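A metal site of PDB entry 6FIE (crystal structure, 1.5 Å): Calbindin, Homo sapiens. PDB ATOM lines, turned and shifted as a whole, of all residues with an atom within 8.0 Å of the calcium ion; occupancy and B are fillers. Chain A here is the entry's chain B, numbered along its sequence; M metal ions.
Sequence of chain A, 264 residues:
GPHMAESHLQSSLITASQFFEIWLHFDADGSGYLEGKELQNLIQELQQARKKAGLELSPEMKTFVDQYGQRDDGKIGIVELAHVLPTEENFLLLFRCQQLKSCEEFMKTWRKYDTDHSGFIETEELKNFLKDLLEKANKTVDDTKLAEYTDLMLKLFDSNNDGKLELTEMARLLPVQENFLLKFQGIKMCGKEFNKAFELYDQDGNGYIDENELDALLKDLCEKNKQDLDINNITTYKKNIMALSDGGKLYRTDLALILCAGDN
The backbone NH of His 117 sits close to the side-chain carboxylate of Asp 114.
OD2 of Asp 114 sits at hydrogen-bond distance from N of Gly 119 (2.9 Å).
N of Thr 115 lies close to OE2 of Glu 125, at 3.3 Å.
Of the 16 residues printed, 6 come within 4 Å of the calcium ion.
The nearest printed residue that does not touch the calcium ion is Ile 121 (4.5 Å).
The calcium ion is bound by OD1 of Asp 114 (2.3 Å), OE1 of Glu 122 (2.3 Å), OD1 of Asp 116 (2.4 Å), OE1 of Glu 125 (2.4 Å), O of Phe 120 (2.4 Å), OG of Ser 118 (2.5 Å) and OE2 of Glu 125 (2.5 Å).
The calcium ion has seven donor atoms within binding distance.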
ATOM      1  N   TRP A 110      30.100 -16.362   2.113  1.00  0.00           N
ATOM      2  CA  TRP A 110      29.577 -15.003   2.109  1.00  0.00           C
ATOM      3  C   TRP A 110      30.050 -14.308   0.821  1.00  0.00           C
ATOM      4  O   TRP A 110      29.240 -13.773   0.088  1.00  0.00           O
ATOM      5  CB  TRP A 110      30.066 -14.236   3.341  1.00  0.00           C
ATOM      6  CG  TRP A 110      29.683 -12.794   3.287  1.00  0.00           C
ATOM      7  CD1 TRP A 110      30.344 -11.769   2.669  1.00  0.00           C
ATOM      8  CD2 TRP A 110      28.482 -12.246   3.785  1.00  0.00           C
ATOM      9  NE1 TRP A 110      29.640 -10.609   2.793  1.00  0.00           N
ATOM     10  CE2 TRP A 110      28.475 -10.874   3.457  1.00  0.00           C
ATOM     11  CE3 TRP A 110      27.384 -12.777   4.466  1.00  0.00           C
ATOM     12  CZ2 TRP A 110      27.428 -10.034   3.808  1.00  0.00           C
ATOM     13  CZ3 TRP A 110      26.400 -11.932   4.895  1.00  0.00           C
ATOM     14  CH2 TRP A 110      26.405 -10.580   4.527  1.00  0.00           C
ATOM     15  N   TYR A 113      28.243 -15.703  -2.366  1.00  0.00           N
ATOM     16  CA  TYR A 113      26.834 -15.429  -2.558  1.00  0.00           C
ATOM     17  C   TYR A 113      26.433 -13.953  -2.539  1.00  0.00           C
ATOM     18  O   TYR A 113      25.339 -13.648  -3.006  1.00  0.00           O
ATOM     19  CB  TYR A 113      26.001 -16.241  -1.576  1.00  0.00           C
ATOM     20  CG  TYR A 113      25.950 -17.687  -1.979  1.00  0.00           C
ATOM     21  CD1 TYR A 113      25.103 -18.117  -2.991  1.00  0.00           C
ATOM     22  CD2 TYR A 113      26.848 -18.606  -1.462  1.00  0.00           C
ATOM     23  CE1 TYR A 113      25.127 -19.431  -3.459  1.00  0.00           C
ATOM     24  CE2 TYR A 113      26.859 -19.941  -1.896  1.00  0.00           C
ATOM     25  CZ  TYR A 113      25.969 -20.350  -2.880  1.00  0.00           C
ATOM     26  OH  TYR A 113      26.005 -21.654  -3.330  1.00  0.00           O
ATOM     27  N   ASP A 114      27.315 -13.032  -2.110  1.00  0.00           N
ATOM     28  CA  ASP A 114      27.044 -11.589  -2.251  1.00  0.00           C
ATOM     29  C   ASP A 114      27.427 -11.201  -3.686  1.00  0.00           C
ATOM     30  O   ASP A 114      28.423 -10.488  -3.927  1.00  0.00           O
ATOM     31  CB  ASP A 114      27.760 -10.768  -1.178  1.00  0.00           C
ATOM     32  CG  ASP A 114      27.518  -9.261  -1.359  1.00  0.00           C
ATOM     33  OD1 ASP A 114      26.536  -8.896  -1.993  1.00  0.00           O
ATOM     34  OD2 ASP A 114      28.296  -8.478  -0.807  1.00  0.00           O
ATOM     35  N   THR A 115      26.627 -11.634  -4.663  1.00  0.00           N
ATOM     36  CA  THR A 115      26.982 -11.516  -6.073  1.00  0.00           C
ATOM     37  C   THR A 115      26.852 -10.121  -6.618  1.00  0.00           C
ATOM     38  O   THR A 115      27.392  -9.886  -7.721  1.00  0.00           O
ATOM     39  CB  THR A 115      26.208 -12.513  -6.902  1.00  0.00           C
ATOM     40  OG1 THR A 115      24.824 -12.453  -6.534  1.00  0.00           O
ATOM     41  CG2 THR A 115      26.698 -13.929  -6.693  1.00  0.00           C
ATOM     42  N   ASP A 116      26.148  -9.200  -5.926  1.00  0.00           N
ATOM     43  CA  ASP A 116      26.076  -7.840  -6.386  1.00  0.00           C
ATOM     44  C   ASP A 116      27.046  -6.923  -5.603  1.00  0.00           C
ATOM     45  O   ASP A 116      26.981  -5.698  -5.728  1.00  0.00           O
ATOM     46  CB  ASP A 116      24.662  -7.292  -6.343  1.00  0.00           C
ATOM     47  CG  ASP A 116      24.085  -7.065  -4.981  1.00  0.00           C
ATOM     48  OD1 ASP A 116      24.710  -7.539  -4.005  1.00  0.00           O
ATOM     49  OD2 ASP A 116      23.036  -6.361  -4.900  1.00  0.00           O
ATOM     50  N   HIS A 117      27.883  -7.493  -4.734  1.00  0.00           N
ATOM     51  CA  HIS A 117      28.889  -6.772  -3.981  1.00  0.00           C
ATOM     52  C   HIS A 117      28.231  -5.678  -3.164  1.00  0.00           C
ATOM     53  O   HIS A 117      28.795  -4.559  -3.035  1.00  0.00           O
ATOM     54  CB  HIS A 117      29.974  -6.192  -4.923  1.00  0.00           C
ATOM     55  CG  HIS A 117      30.725  -7.199  -5.727  1.00  0.00           C
ATOM     56  ND1 HIS A 117      31.721  -6.813  -6.611  1.00  0.00           N
ATOM     57  CD2 HIS A 117      30.664  -8.553  -5.731  1.00  0.00           C
ATOM     58  CE1 HIS A 117      32.201  -7.929  -7.123  1.00  0.00           C
ATOM     59  NE2 HIS A 117      31.611  -8.999  -6.611  1.00  0.00           N
ATOM     60  N   SER A 118      27.036  -5.949  -2.603  1.00  0.00           N
ATOM     61  CA  SER A 118      26.355  -4.921  -1.796  1.00  0.00           C
ATOM     62  C   SER A 118      26.808  -4.846  -0.362  1.00  0.00           C
ATOM     63  O   SER A 118      26.430  -3.897   0.326  1.00  0.00           O
ATOM     64  CB  SER A 118      24.862  -5.117  -1.822  1.00  0.00           C
ATOM     65  OG  SER A 118      24.507  -6.321  -1.162  1.00  0.00           O
ATOM     66  N   GLY A 119      27.509  -5.862   0.087  1.00  0.00           N
ATOM     67  CA  GLY A 119      27.901  -5.987   1.476  1.00  0.00           C
ATOM     68  C   GLY A 119      26.823  -6.563   2.358  1.00  0.00           C
ATOM     69  O   GLY A 119      26.981  -6.572   3.586  1.00  0.00           O
ATOM     70  N   PHE A 120      25.774  -7.074   1.770  1.00  0.00           N
ATOM     71  CA  PHE A 120      24.689  -7.779   2.485  1.00  0.00           C
ATOM     72  C   PHE A 120      24.231  -8.939   1.648  1.00  0.00           C
ATOM     73  O   PHE A 120      24.352  -8.898   0.444  1.00  0.00           O
ATOM     74  CB  PHE A 120      23.458  -6.920   2.703  1.00  0.00           C
ATOM     75  CG  PHE A 120      23.682  -5.643   3.477  1.00  0.00           C
ATOM     76  CD1 PHE A 120      23.634  -5.639   4.875  1.00  0.00           C
ATOM     77  CD2 PHE A 120      23.948  -4.456   2.829  1.00  0.00           C
ATOM     78  CE1 PHE A 120      23.844  -4.442   5.604  1.00  0.00           C
ATOM     79  CE2 PHE A 120      24.176  -3.268   3.551  1.00  0.00           C
ATOM     80  CZ  PHE A 120      24.130  -3.277   4.927  1.00  0.00           C
ATOM     81  N   ILE A 121      23.630  -9.935   2.287  1.00  0.00           N
ATOM     82  CA  ILE A 121      22.959 -11.035   1.605  1.00  0.00           C
ATOM     83  C   ILE A 121      21.463 -10.701   1.580  1.00  0.00           C
ATOM     84  O   ILE A 121      20.791 -10.727   2.637  1.00  0.00           O
ATOM     85  CB  ILE A 121      23.289 -12.399   2.234  1.00  0.00           C
ATOM     86  CG1 ILE A 121      24.741 -12.778   2.018  1.00  0.00           C
ATOM     87  CG2 ILE A 121      22.332 -13.499   1.738  1.00  0.00           C
ATOM     88  CD1 ILE A 121      25.142 -13.094   0.579  1.00  0.00           C
ATOM     89  N   GLU A 122      20.948 -10.332   0.404  1.00  0.00           N
ATOM     90  CA  GLU A 122      19.534 -10.015   0.169  1.00  0.00           C
ATOM     91  C   GLU A 122      18.741 -11.318  -0.080  1.00  0.00           C
ATOM     92  O   GLU A 122      19.341 -12.369  -0.261  1.00  0.00           O
ATOM     93  CB  GLU A 122      19.351  -8.994  -0.968  1.00  0.00           C
ATOM     94  CG  GLU A 122      19.934  -7.614  -0.626  1.00  0.00           C
ATOM     95  CD  GLU A 122      21.399  -7.384  -0.933  1.00  0.00           C
ATOM     96  OE1 GLU A 122      21.958  -8.123  -1.765  1.00  0.00           O
ATOM     97  OE2 GLU A 122      21.953  -6.403  -0.386  1.00  0.00           O
ATOM     98  N   THR A 123      17.408 -11.252  -0.065  1.00  0.00           N
ATOM     99  CA  THR A 123      16.532 -12.414  -0.174  1.00  0.00           C
ATOM    100  C   THR A 123      16.871 -13.328  -1.330  1.00  0.00           C
ATOM    101  O   THR A 123      16.951 -14.556  -1.144  1.00  0.00           O
ATOM    102  CB  THR A 123      15.049 -11.954  -0.281  1.00  0.00           C
ATOM    103  OG1 THR A 123      14.819 -11.067   0.805  1.00  0.00           O
ATOM    104  CG2 THR A 123      14.078 -13.096  -0.178  1.00  0.00           C
ATOM    105  N   GLU A 125      19.675 -13.695  -2.961  1.00  0.00           N
ATOM    106  CA  GLU A 125      20.971 -14.318  -2.761  1.00  0.00           C
ATOM    107  C   GLU A 125      20.861 -15.457  -1.721  1.00  0.00           C
ATOM    108  O   GLU A 125      21.520 -16.496  -1.820  1.00  0.00           O
ATOM    109  CB  GLU A 125      22.023 -13.260  -2.308  1.00  0.00           C
ATOM    110  CG  GLU A 125      22.345 -12.246  -3.377  1.00  0.00           C
ATOM    111  CD  GLU A 125      23.214 -11.092  -2.904  1.00  0.00           C
ATOM    112  OE1 GLU A 125      23.275 -10.864  -1.666  1.00  0.00           O
ATOM    113  OE2 GLU A 125      23.760 -10.351  -3.764  1.00  0.00           O
ATOM    114  N   LEU A 126      20.086 -15.222  -0.672  1.00  0.00           N
ATOM    115  CA  LEU A 126      19.883 -16.225   0.343  1.00  0.00           C
ATOM    116  C   LEU A 126      19.140 -17.433  -0.282  1.00  0.00           C
ATOM    117  O   LEU A 126      19.568 -18.572  -0.082  1.00  0.00           O
ATOM    118  CB  LEU A 126      19.075 -15.617   1.500  1.00  0.00           C
ATOM    119  CG  LEU A 126      18.839 -16.572   2.674  1.00  0.00           C
ATOM    120  CD1 LEU A 126      20.158 -17.127   3.280  1.00  0.00           C
ATOM    121  CD2 LEU A 126      17.955 -15.902   3.728  1.00  0.00           C
ATOM    122  N   LYS A 164      17.373  -7.867   5.171  1.00  0.00           N
ATOM    123  CA  LYS A 164      18.578  -8.470   4.571  1.00  0.00           C
ATOM    124  C   LYS A 164      19.568  -8.839   5.658  1.00  0.00           C
ATOM    125  O   LYS A 164      19.466  -8.373   6.798  1.00  0.00           O
ATOM    126  CB  LYS A 164      19.226  -7.526   3.537  1.00  0.00           C
ATOM    127  CG  LYS A 164      19.702  -6.205   4.132  1.00  0.00           C
ATOM    128  CD  LYS A 164      19.895  -5.147   3.070  1.00  0.00           C
ATOM    129  CE  LYS A 164      20.276  -3.849   3.736  1.00  0.00           C
ATOM    130  NZ  LYS A 164      20.519  -2.771   2.737  1.00  0.00           N
ATOM    131  N   LEU A 165      20.514  -9.736   5.340  1.00  0.00           N
ATOM    132  CA  LEU A 165      21.469 -10.223   6.293  1.00  0.00           C
ATOM    133  C   LEU A 165      22.794  -9.534   6.145  1.00  0.00           C
ATOM    134  O   LEU A 165      23.292  -9.468   5.032  1.00  0.00           O
ATOM    135  CB  LEU A 165      21.676 -11.749   6.165  1.00  0.00           C
ATOM    136  CG  LEU A 165      20.414 -12.579   6.395  1.00  0.00           C
ATOM    137  CD1 LEU A 165      20.687 -14.094   6.199  1.00  0.00           C
ATOM    138  CD2 LEU A 165      19.845 -12.342   7.790  1.00  0.00           C
HETATM  139 CA    CA M   1      24.218  -8.663  -1.965  1.00  0.00          CA
